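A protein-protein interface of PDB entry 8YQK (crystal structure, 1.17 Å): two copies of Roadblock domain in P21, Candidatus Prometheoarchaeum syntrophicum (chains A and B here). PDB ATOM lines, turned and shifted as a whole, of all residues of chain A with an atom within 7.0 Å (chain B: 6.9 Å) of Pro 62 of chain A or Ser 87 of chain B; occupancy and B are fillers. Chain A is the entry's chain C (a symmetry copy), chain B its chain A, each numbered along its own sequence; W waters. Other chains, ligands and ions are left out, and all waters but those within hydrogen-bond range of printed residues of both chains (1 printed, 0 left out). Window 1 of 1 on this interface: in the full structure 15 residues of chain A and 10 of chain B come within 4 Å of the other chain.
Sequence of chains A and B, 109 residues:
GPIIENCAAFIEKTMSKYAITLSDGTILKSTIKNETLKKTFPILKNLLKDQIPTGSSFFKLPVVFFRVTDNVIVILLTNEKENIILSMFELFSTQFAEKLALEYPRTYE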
ATOM      1  N   ILE A  32      26.713 -12.119  -5.472  1.00  0.00           N
ATOM      2  CA  ILE A  32      26.726 -12.914  -4.249  1.00  0.00           C
ATOM      3  C   ILE A  32      27.092 -14.336  -4.638  1.00  0.00           C
ATOM      4  O   ILE A  32      26.648 -14.836  -5.680  1.00  0.00           O
ATOM      5  CB  ILE A  32      25.335 -12.863  -3.596  1.00  0.00           C
ATOM      6  CG1 ILE A  32      25.007 -11.427  -3.165  1.00  0.00           C
ATOM      7  CG2 ILE A  32      25.241 -13.835  -2.391  1.00  0.00           C
ATOM      8  CD1 ILE A  32      23.547 -11.195  -2.796  1.00  0.00           C
ATOM      9  N   THR A  36      25.886 -19.037  -1.050  1.00  0.00           N
ATOM     10  CA  THR A  36      25.269 -18.099  -0.120  1.00  0.00           C
ATOM     11  C   THR A  36      23.878 -17.714  -0.598  1.00  0.00           C
ATOM     12  O   THR A  36      22.907 -17.725   0.167  1.00  0.00           O
ATOM     13  CB  THR A  36      26.162 -16.862   0.008  1.00  0.00           C
ATOM     14  OG1 THR A  36      27.520 -17.270   0.220  1.00  0.00           O
ATOM     15  CG2 THR A  36      25.704 -15.976   1.153  1.00  0.00           C
ATOM     16  N   LEU A  37      23.753 -17.424  -1.890  1.00  0.00           N
ATOM     17  CA  LEU A  37      22.467 -17.022  -2.436  1.00  0.00           C
ATOM     18  C   LEU A  37      21.449 -18.155  -2.330  1.00  0.00           C
ATOM     19  O   LEU A  37      20.296 -17.926  -1.943  1.00  0.00           O
ATOM     20  CB  LEU A  37      22.678 -16.545  -3.876  1.00  0.00           C
ATOM     21  CG  LEU A  37      21.518 -15.848  -4.553  1.00  0.00           C
ATOM     22  CD1 LEU A  37      21.156 -14.607  -3.754  1.00  0.00           C
ATOM     23  CD2 LEU A  37      21.935 -15.490  -5.970  1.00  0.00           C
ATOM     24  N   LYS A  39      21.244 -20.420  -0.105  1.00  0.00           N
ATOM     25  CA  LYS A  39      20.806 -20.613   1.275  1.00  0.00           C
ATOM     26  C   LYS A  39      19.743 -19.602   1.698  1.00  0.00           C
ATOM     27  O   LYS A  39      18.947 -19.892   2.598  1.00  0.00           O
ATOM     28  CB  LYS A  39      22.005 -20.567   2.227  1.00  0.00           C
ATOM     29  CG  LYS A  39      22.144 -21.792   3.121  1.00  0.00           C
ATOM     30  CD  LYS A  39      22.360 -23.065   2.322  1.00  0.00           C
ATOM     31  CE  LYS A  39      23.838 -23.343   2.112  1.00  0.00           C
ATOM     32  NZ  LYS A  39      24.191 -24.744   2.479  1.00  0.00           N
ATOM     33  N   THR A  40      19.712 -18.423   1.069  1.00  0.00           N
ATOM     34  CA  THR A  40      18.727 -17.401   1.420  1.00  0.00           C
ATOM     35  C   THR A  40      17.359 -17.650   0.795  1.00  0.00           C
ATOM     36  O   THR A  40      16.368 -17.078   1.260  1.00  0.00           O
ATOM     37  CB  THR A  40      19.221 -16.002   1.026  1.00  0.00           C
ATOM     38  OG1 THR A  40      19.064 -15.796  -0.387  1.00  0.00           O
ATOM     39  CG2 THR A  40      20.685 -15.825   1.416  1.00  0.00           C
ATOM     40  N   PHE A  59      13.915  -6.559   5.585  1.00  0.00           N
ATOM     41  CA  PHE A  59      15.278  -6.439   6.096  1.00  0.00           C
ATOM     42  C   PHE A  59      15.547  -7.547   7.101  1.00  0.00           C
ATOM     43  O   PHE A  59      14.878  -7.623   8.137  1.00  0.00           O
ATOM     44  CB  PHE A  59      15.474  -5.084   6.777  1.00  0.00           C
ATOM     45  CG  PHE A  59      15.507  -3.930   5.820  1.00  0.00           C
ATOM     46  CD1 PHE A  59      14.341  -3.478   5.229  1.00  0.00           C
ATOM     47  CD2 PHE A  59      16.695  -3.302   5.490  1.00  0.00           C
ATOM     48  CE1 PHE A  59      14.352  -2.417   4.336  1.00  0.00           C
ATOM     49  CE2 PHE A  59      16.713  -2.237   4.596  1.00  0.00           C
ATOM     50  CZ  PHE A  59      15.535  -1.798   4.019  1.00  0.00           C
ATOM     51  N   LYS A  60      16.540  -8.390   6.803  1.00  0.00           N
ATOM     52  CA  LYS A  60      16.988  -9.453   7.688  1.00  0.00           C
ATOM     53  C   LYS A  60      18.518  -9.401   7.660  1.00  0.00           C
ATOM     54  O   LYS A  60      19.189 -10.239   7.053  1.00  0.00           O
ATOM     55  CB  LYS A  60      16.460 -10.811   7.222  1.00  0.00           C
ATOM     56  CG  LYS A  60      16.482 -11.896   8.278  1.00  0.00           C
ATOM     57  CD  LYS A  60      15.743 -13.124   7.772  1.00  0.00           C
ATOM     58  CE  LYS A  60      16.188 -14.373   8.500  1.00  0.00           C
ATOM     59  NZ  LYS A  60      15.795 -14.316   9.935  1.00  0.00           N
ATOM     60  N   LEU A  61      19.080  -8.403   8.341  1.00  0.00           N
ATOM     61  CA  LEU A  61      20.430  -7.956   8.025  1.00  0.00           C
ATOM     62  C   LEU A  61      21.454  -9.075   8.188  1.00  0.00           C
ATOM     63  O   LEU A  61      21.423  -9.810   9.188  1.00  0.00           O
ATOM     64  CB  LEU A  61      20.833  -6.767   8.892  1.00  0.00           C
ATOM     65  CG  LEU A  61      20.179  -5.429   8.554  1.00  0.00           C
ATOM     66  CD1 LEU A  61      20.784  -4.365   9.473  1.00  0.00           C
ATOM     67  CD2 LEU A  61      20.345  -5.064   7.082  1.00  0.00           C
ATOM     68  N   PRO A  62      22.407  -9.181   7.279  1.00  0.00           N
ATOM     69  CA  PRO A  62      22.684  -8.242   6.178  1.00  0.00           C
ATOM     70  C   PRO A  62      21.865  -8.449   4.924  1.00  0.00           C
ATOM     71  O   PRO A  62      22.073  -7.735   3.943  1.00  0.00           O
ATOM     72  CB  PRO A  62      24.168  -8.510   5.883  1.00  0.00           C
ATOM     73  CG  PRO A  62      24.289 -10.006   6.115  1.00  0.00           C
ATOM     74  CD  PRO A  62      23.408 -10.273   7.326  1.00  0.00           C
ATOM     75  N   VAL A  63      20.955  -9.412   4.908  1.00  0.00           N
ATOM     76  CA  VAL A  63      20.135  -9.671   3.725  1.00  0.00           C
ATOM     77  C   VAL A  63      18.978  -8.682   3.651  1.00  0.00           C
ATOM     78  O   VAL A  63      18.270  -8.455   4.638  1.00  0.00           O
ATOM     79  CB  VAL A  63      19.646 -11.121   3.726  1.00  0.00           C
ATOM     80  CG1 VAL A  63      18.937 -11.432   2.416  1.00  0.00           C
ATOM     81  CG2 VAL A  63      20.816 -12.087   3.928  1.00  0.00           C
ATOM     82  N   VAL A  64      18.795  -8.077   2.475  1.00  0.00           N
ATOM     83  CA  VAL A  64      17.646  -7.222   2.204  1.00  0.00           C
ATOM     84  C   VAL A  64      16.996  -7.689   0.916  1.00  0.00           C
ATOM     85  O   VAL A  64      17.686  -7.911  -0.087  1.00  0.00           O
ATOM     86  CB  VAL A  64      18.052  -5.742   2.104  1.00  0.00           C
ATOM     87  CG1 VAL A  64      16.809  -4.868   1.949  1.00  0.00           C
ATOM     88  CG2 VAL A  64      18.853  -5.330   3.339  1.00  0.00           C
ATOM     89  N   LEU A  76      20.087  -7.760  -1.635  1.00  0.00           N
ATOM     90  CA  LEU A  76      21.359  -7.145  -1.272  1.00  0.00           C
ATOM     91  C   LEU A  76      21.948  -7.865  -0.072  1.00  0.00           C
ATOM     92  O   LEU A  76      21.215  -8.397   0.765  1.00  0.00           O
ATOM     93  CB  LEU A  76      21.163  -5.712  -0.811  1.00  0.00           C
ATOM     94  CG  LEU A  76      20.446  -4.748  -1.736  1.00  0.00           C
ATOM     95  CD1 LEU A  76      20.404  -3.357  -1.072  1.00  0.00           C
ATOM     96  CD2 LEU A  76      21.106  -4.708  -3.111  1.00  0.00           C
ATOM     97  N   LEU A  77      23.282  -7.833   0.026  1.00  0.00           N
ATOM     98  CA  LEU A  77      23.959  -8.000   1.309  1.00  0.00           C
ATOM     99  C   LEU A  77      24.503  -6.623   1.664  1.00  0.00           C
ATOM    100  O   LEU A  77      25.311  -6.070   0.918  1.00  0.00           O
ATOM    101  CB  LEU A  77      25.123  -8.987   1.216  1.00  0.00           C
ATOM    102  CG  LEU A  77      24.818 -10.408   0.750  1.00  0.00           C
ATOM    103  CD1 LEU A  77      26.044 -11.297   0.883  1.00  0.00           C
ATOM    104  CD2 LEU A  77      23.614 -11.017   1.433  1.00  0.00           C
ATOM    105  N   THR A  78      24.084  -6.078   2.800  1.00  0.00           N
ATOM    106  CA  THR A  78      24.476  -4.706   3.091  1.00  0.00           C
ATOM    107  C   THR A  78      24.394  -4.427   4.584  1.00  0.00           C
ATOM    108  O   THR A  78      23.683  -5.100   5.331  1.00  0.00           O
ATOM    109  CB  THR A  78      23.592  -3.720   2.315  1.00  0.00           C
ATOM    110  OG1 THR A  78      24.075  -2.385   2.527  1.00  0.00           O
ATOM    111  CG2 THR A  78      22.143  -3.822   2.765  1.00  0.00           C
ATOM    112  N   ASN A  79      25.190  -3.436   5.004  1.00  0.00           N
ATOM    113  CA  ASN A  79      25.136  -2.853   6.338  1.00  0.00           C
ATOM    114  C   ASN A  79      24.908  -1.344   6.242  1.00  0.00           C
ATOM    115  O   ASN A  79      25.175  -0.608   7.200  1.00  0.00           O
ATOM    116  CB  ASN A  79      26.424  -3.172   7.114  1.00  0.00           C
ATOM    117  CG  ASN A  79      26.283  -2.986   8.622  1.00  0.00           C
ATOM    118  OD1 ASN A  79      25.244  -3.296   9.205  1.00  0.00           O
ATOM    119  ND2 ASN A  79      27.332  -2.473   9.256  1.00  0.00           N
ATOM    120  N   PHE B  10      30.787  -4.092  12.911  1.00  0.00           N
ATOM    121  CA  PHE B  10      30.036  -4.800  11.886  1.00  0.00           C
ATOM    122  C   PHE B  10      29.390  -6.051  12.452  1.00  0.00           C
ATOM    123  O   PHE B  10      28.188  -6.275  12.275  1.00  0.00           O
ATOM    124  CB  PHE B  10      30.979  -5.168  10.743  1.00  0.00           C
ATOM    125  CG  PHE B  10      30.324  -5.934   9.621  1.00  0.00           C
ATOM    126  CD1 PHE B  10      30.119  -7.301   9.708  1.00  0.00           C
ATOM    127  CD2 PHE B  10      29.947  -5.285   8.451  1.00  0.00           C
ATOM    128  CE1 PHE B  10      29.534  -8.001   8.663  1.00  0.00           C
ATOM    129  CE2 PHE B  10      29.389  -5.987   7.395  1.00  0.00           C
ATOM    130  CZ  PHE B  10      29.166  -7.342   7.503  1.00  0.00           C
ATOM    131  N   THR B  14      24.491  -7.490  14.559  1.00  0.00           N
ATOM    132  CA  THR B  14      23.569  -8.610  14.675  1.00  0.00           C
ATOM    133  C   THR B  14      23.973  -9.705  15.660  1.00  0.00           C
ATOM    134  O   THR B  14      23.125 -10.538  15.998  1.00  0.00           O
ATOM    135  CB  THR B  14      23.291  -9.239  13.294  1.00  0.00           C
ATOM    136  OG1 THR B  14      24.487  -9.858  12.806  1.00  0.00           O
ATOM    137  CG2 THR B  14      22.824  -8.187  12.285  1.00  0.00           C
ATOM    138  N   MET B  15      25.229  -9.751  16.113  1.00  0.00           N
ATOM    139  CA  MET B  15      25.722 -10.820  16.981  1.00  0.00           C
ATOM    140  C   MET B  15      26.497 -10.213  18.139  1.00  0.00           C
ATOM    141  O   MET B  15      27.394  -9.395  17.914  1.00  0.00           O
ATOM    142  CB  MET B  15      26.691 -11.745  16.231  1.00  0.00           C
ATOM    143  CG  MET B  15      26.344 -12.046  14.801  1.00  0.00           C
ATOM    144  SD  MET B  15      25.830 -13.759  14.644  1.00  0.00           S
ATOM    145  CE  MET B  15      24.930 -13.676  13.103  1.00  0.00           C
ATOM    146  N   GLU B  82      22.161 -20.757   9.820  1.00  0.00           N
ATOM    147  CA  GLU B  82      23.290 -20.825   8.898  1.00  0.00           C
ATOM    148  C   GLU B  82      23.183 -19.836   7.744  1.00  0.00           C
ATOM    149  O   GLU B  82      24.178 -19.207   7.370  1.00  0.00           O
ATOM    150  CB  GLU B  82      23.430 -22.251   8.359  1.00  0.00           C
ATOM    151  CG  GLU B  82      24.664 -22.456   7.496  1.00  0.00           C
ATOM    152  CD  GLU B  82      24.817 -23.889   7.024  1.00  0.00           C
ATOM    153  OE1 GLU B  82      23.913 -24.706   7.299  1.00  0.00           O
ATOM    154  OE2 GLU B  82      25.840 -24.199   6.376  1.00  0.00           O
ATOM    155  N   ASN B  83      21.990 -19.681   7.160  1.00  0.00           N
ATOM    156  CA  ASN B  83      21.891 -18.876   5.943  1.00  0.00           C
ATOM    157  C   ASN B  83      22.277 -17.422   6.203  1.00  0.00           C
ATOM    158  O   ASN B  83      23.042 -16.821   5.436  1.00  0.00           O
ATOM    159  CB  ASN B  83      20.497 -18.970   5.320  1.00  0.00           C
ATOM    160  CG  ASN B  83      19.465 -18.151   6.067  1.00  0.00           C
ATOM    161  OD1 ASN B  83      19.164 -18.416   7.231  1.00  0.00           O
ATOM    162  ND2 ASN B  83      18.973 -17.104   5.420  1.00  0.00           N
ATOM    163  N   ILE B  84      21.763 -16.841   7.290  1.00  0.00           N
ATOM    164  CA  ILE B  84      22.130 -15.473   7.640  1.00  0.00           C
ATOM    165  C   ILE B  84      23.598 -15.386   8.044  1.00  0.00           C
ATOM    166  O   ILE B  84      24.284 -14.401   7.728  1.00  0.00           O
ATOM    167  CB  ILE B  84      21.184 -14.901   8.711  1.00  0.00           C
ATOM    168  CG1 ILE B  84      19.743 -14.958   8.211  1.00  0.00           C
ATOM    169  CG2 ILE B  84      21.573 -13.477   9.083  1.00  0.00           C
ATOM    170  CD1 ILE B  84      19.550 -14.148   6.949  1.00  0.00           C
ATOM    171  N   ILE B  85      24.106 -16.401   8.750  1.00  0.00           N
ATOM    172  CA  ILE B  85      25.509 -16.391   9.149  1.00  0.00           C
ATOM    173  C   ILE B  85      26.423 -16.376   7.933  1.00  0.00           C
ATOM    174  O   ILE B  85      27.377 -15.588   7.866  1.00  0.00           O
ATOM    175  CB  ILE B  85      25.818 -17.569  10.090  1.00  0.00           C
ATOM    176  CG1 ILE B  85      25.005 -17.464  11.388  1.00  0.00           C
ATOM    177  CG2 ILE B  85      27.316 -17.628  10.404  1.00  0.00           C
ATOM    178  CD1 ILE B  85      24.873 -18.775  12.158  1.00  0.00           C
ATOM    179  N   LEU B  86      26.129 -17.210   6.933  1.00  0.00           N
ATOM    180  CA  LEU B  86      26.971 -17.256   5.742  1.00  0.00           C
ATOM    181  C   LEU B  86      26.969 -15.907   5.032  1.00  0.00           C
ATOM    182  O   LEU B  86      28.001 -15.467   4.508  1.00  0.00           O
ATOM    183  CB  LEU B  86      26.449 -18.332   4.790  1.00  0.00           C
ATOM    184  CG  LEU B  86      26.704 -19.785   5.202  1.00  0.00           C
ATOM    185  CD1 LEU B  86      26.021 -20.697   4.202  1.00  0.00           C
ATOM    186  CD2 LEU B  86      28.181 -20.123   5.304  1.00  0.00           C
ATOM    187  N   SER B  87      25.803 -15.239   4.994  1.00  0.00           N
ATOM    188  CA  SER B  87      25.711 -13.918   4.370  1.00  0.00           C
ATOM    189  C   SER B  87      26.511 -12.885   5.145  1.00  0.00           C
ATOM    190  O   SER B  87      27.169 -12.022   4.552  1.00  0.00           O
ATOM    191  CB  SER B  87      24.251 -13.473   4.301  1.00  0.00           C
ATOM    192  OG  SER B  87      23.462 -14.387   3.552  1.00  0.00           O
ATOM    193  N   MET B  88      26.466 -12.955   6.472  1.00  0.00           N
ATOM    194  CA  MET B  88      27.264 -12.045   7.282  1.00  0.00           C
ATOM    195  C   MET B  88      28.750 -12.238   6.997  1.00  0.00           C
ATOM    196  O   MET B  88      29.486 -11.267   6.782  1.00  0.00           O
ATOM    197  CB  MET B  88      26.949 -12.270   8.761  1.00  0.00           C
ATOM    198  CG  MET B  88      27.509 -11.192   9.670  1.00  0.00           C
ATOM    199  SD  MET B  88      29.228 -11.437  10.163  1.00  0.00           S
ATOM    200  CE  MET B  88      29.086 -12.753  11.365  1.00  0.00           C
ATOM    201  N   PHE B  89      29.210 -13.495   6.965  1.00  0.00           N
ATOM    202  CA  PHE B  89      30.622 -13.752   6.676  1.00  0.00           C
ATOM    203  C   PHE B  89      31.012 -13.224   5.296  1.00  0.00           C
ATOM    204  O   PHE B  89      32.102 -12.654   5.111  1.00  0.00           O
ATOM    205  CB  PHE B  89      30.912 -15.255   6.713  1.00  0.00           C
ATOM    206  CG  PHE B  89      30.883 -15.888   8.092  1.00  0.00           C
ATOM    207  CD1 PHE B  89      31.119 -15.172   9.250  1.00  0.00           C
ATOM    208  CD2 PHE B  89      30.638 -17.250   8.194  1.00  0.00           C
ATOM    209  CE1 PHE B  89      31.122 -15.832  10.504  1.00  0.00           C
ATOM    210  CE2 PHE B  89      30.639 -17.902   9.427  1.00  0.00           C
ATOM    211  CZ  PHE B  89      30.874 -17.192  10.569  1.00  0.00           C
ATOM    212  N   GLU B  90      30.146 -13.432   4.305  1.00  0.00           N
ATOM    213  CA  GLU B  90      30.478 -13.017   2.948  1.00  0.00           C
ATOM    214  C   GLU B  90      30.637 -11.501   2.861  1.00  0.00           C
ATOM    215  O   GLU B  90      31.615 -10.991   2.288  1.00  0.00           O
ATOM    216  CB  GLU B  90      29.418 -13.532   1.972  1.00  0.00           C
ATOM    217  CG  GLU B  90      29.663 -13.037   0.551  1.00  0.00           C
ATOM    218  CD  GLU B  90      29.263 -14.039  -0.524  1.00  0.00           C
ATOM    219  OE1 GLU B  90      29.358 -15.263  -0.258  1.00  0.00           O
ATOM    220  OE2 GLU B  90      28.857 -13.602  -1.634  1.00  0.00           O
ATOM    221  N   LEU B  91      29.686 -10.758   3.432  1.00  0.00           N
ATOM    222  CA  LEU B  91      29.799  -9.302   3.434  1.00  0.00           C
ATOM    223  C   LEU B  91      30.980  -8.839   4.289  1.00  0.00           C
ATOM    224  O   LEU B  91      31.687  -7.897   3.917  1.00  0.00           O
ATOM    225  CB  LEU B  91      28.498  -8.667   3.921  1.00  0.00           C
ATOM    226  CG  LEU B  91      28.478  -7.136   3.867  1.00  0.00           C
ATOM    227  CD1 LEU B  91      28.631  -6.601   2.440  1.00  0.00           C
ATOM    228  CD2 LEU B  91      27.193  -6.629   4.505  1.00  0.00           C
ATOM    229  N   PHE B  92      31.222  -9.497   5.433  1.00  0.00           N
ATOM    230  CA  PHE B  92      32.372  -9.156   6.276  1.00  0.00           C
ATOM    231  C   PHE B  92      33.667  -9.274   5.491  1.00  0.00           C
ATOM    232  O   PHE B  92      34.516  -8.372   5.517  1.00  0.00           O
ATOM    233  CB  PHE B  92      32.405 -10.101   7.475  1.00  0.00           C
ATOM    234  CG  PHE B  92      33.521  -9.818   8.462  1.00  0.00           C
ATOM    235  CD1 PHE B  92      33.352  -8.913   9.493  1.00  0.00           C
ATOM    236  CD2 PHE B  92      34.749 -10.453   8.342  1.00  0.00           C
ATOM    237  CE1 PHE B  92      34.375  -8.678  10.426  1.00  0.00           C
ATOM    238  CE2 PHE B  92      35.789 -10.208   9.260  1.00  0.00           C
ATOM    239  CZ  PHE B  92      35.609  -9.320  10.292  1.00  0.00           C
ATOM    240  N   SER B  93      33.816 -10.365   4.748  1.00  0.00           N
ATOM    241  CA  SER B  93      35.026 -10.547   3.953  1.00  0.00           C
ATOM    242  C   SER B  93      35.129  -9.484   2.862  1.00  0.00           C
ATOM    243  O   SER B  93      36.197  -8.884   2.641  1.00  0.00           O
ATOM    244  CB  SER B  93      35.020 -11.939   3.345  1.00  0.00           C
ATOM    245  OG  SER B  93      36.222 -12.172   2.644  1.00  0.00           O
HETATM  246  O   HOH W   1      23.424 -11.344  10.741  1.00  0.00           O
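The backbone carbonyl oxygen (O) of Asn 83 of chain B lies within hydrogen-bond range of the side-chain hydroxyl (OG) of Ser 87 of chain B, 3.1 Å away.
The backbone carbonyl oxygen of Leu 37 of chain A is in hydrogen-bond range of the side-chain hydroxyl of Thr 40 of chain A, 2.9 Å away.
The backbone carbonyl oxygen (O) of Pro 62 of chain A sits at hydrogen-bond distance from the backbone NH (N) of Thr 78 of chain A, at 2.8 Å.
Hydrophobic or aromatic side chains of chain B within 4 Å of the printed part of chain A: Phe 10, Ile 84 and Leu 91.
Among the printed residues, 18 pairs touch across the chains.
OE1 of Glu 90 of chain B is in hydrogen-bond range of OG1 of Thr 36 of chain A, 2.8 Å away.
No position is printed for both chains.
Of the 18 pairs that touch across the chains among the printed residues, none has its exchanged pair printed and touching as well.
Printed residues of chain B within 4 Å of Leu 61 of chain A: Thr 14 and Ile 84.
Printed residues of chain B within 4 Å of Thr 78 of chain A: Leu 91 (3.6 Å).
Printed residues of chain B within 4 Å of Asn 79 of chain A: Phe 10 and Leu 91.
Of the printed residues of chain A, Ile 84 of chain B touches Lys 60 (3.6 Å), Leu 61 (3.7 Å) and Val 63 (3.9 Å).
Of the printed residues of chain A, Asn 83 of chain B touches Lys 39.
Leu 37 of chain A touches none of the printed residues of chain B.
The nearest printed residue of chain B that does not touch Pro 62 of chain A is Ile 84 of chain B (4.1 Å).
The nearest printed residue of chain B that does not touch Lys 60 of chain A is Asn 83 of chain B (5.0 Å).
Water W1 bridges OG1 of Thr 14 of chain B (2.8 Å) and O of Leu 61 of chain A (3.0 Å).
Ile 32 of chain A touches Glu 90 of chain B (CA to OE2, 3.4 Å).
Ser 87 of chain B touches Thr 40 of chain A.
Lys 60 of chain A touches Ile 84 of chain B (CE to CG1, 3.6 Å).
Leu 61 of chain A touches Thr 14 of chain B (O to CG2, 3.8 Å).
CB of Pro 62 of chain A touches CD2 of Leu 91 of chain B (3.8 Å).
Ser 87 of chain B touches Val 63 of chain A.
Leu 77 of chain A touches Ser 87 of chain B.
Leu 91 of chain B touches Leu 77 of chain A (CD1 to O, 3.7 Å).
Asn 79 of chain A touches Phe 10 of chain B (ND2 to CD2, 3.9 Å).
Asn 79 of chain A touches Leu 91 of chain B.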
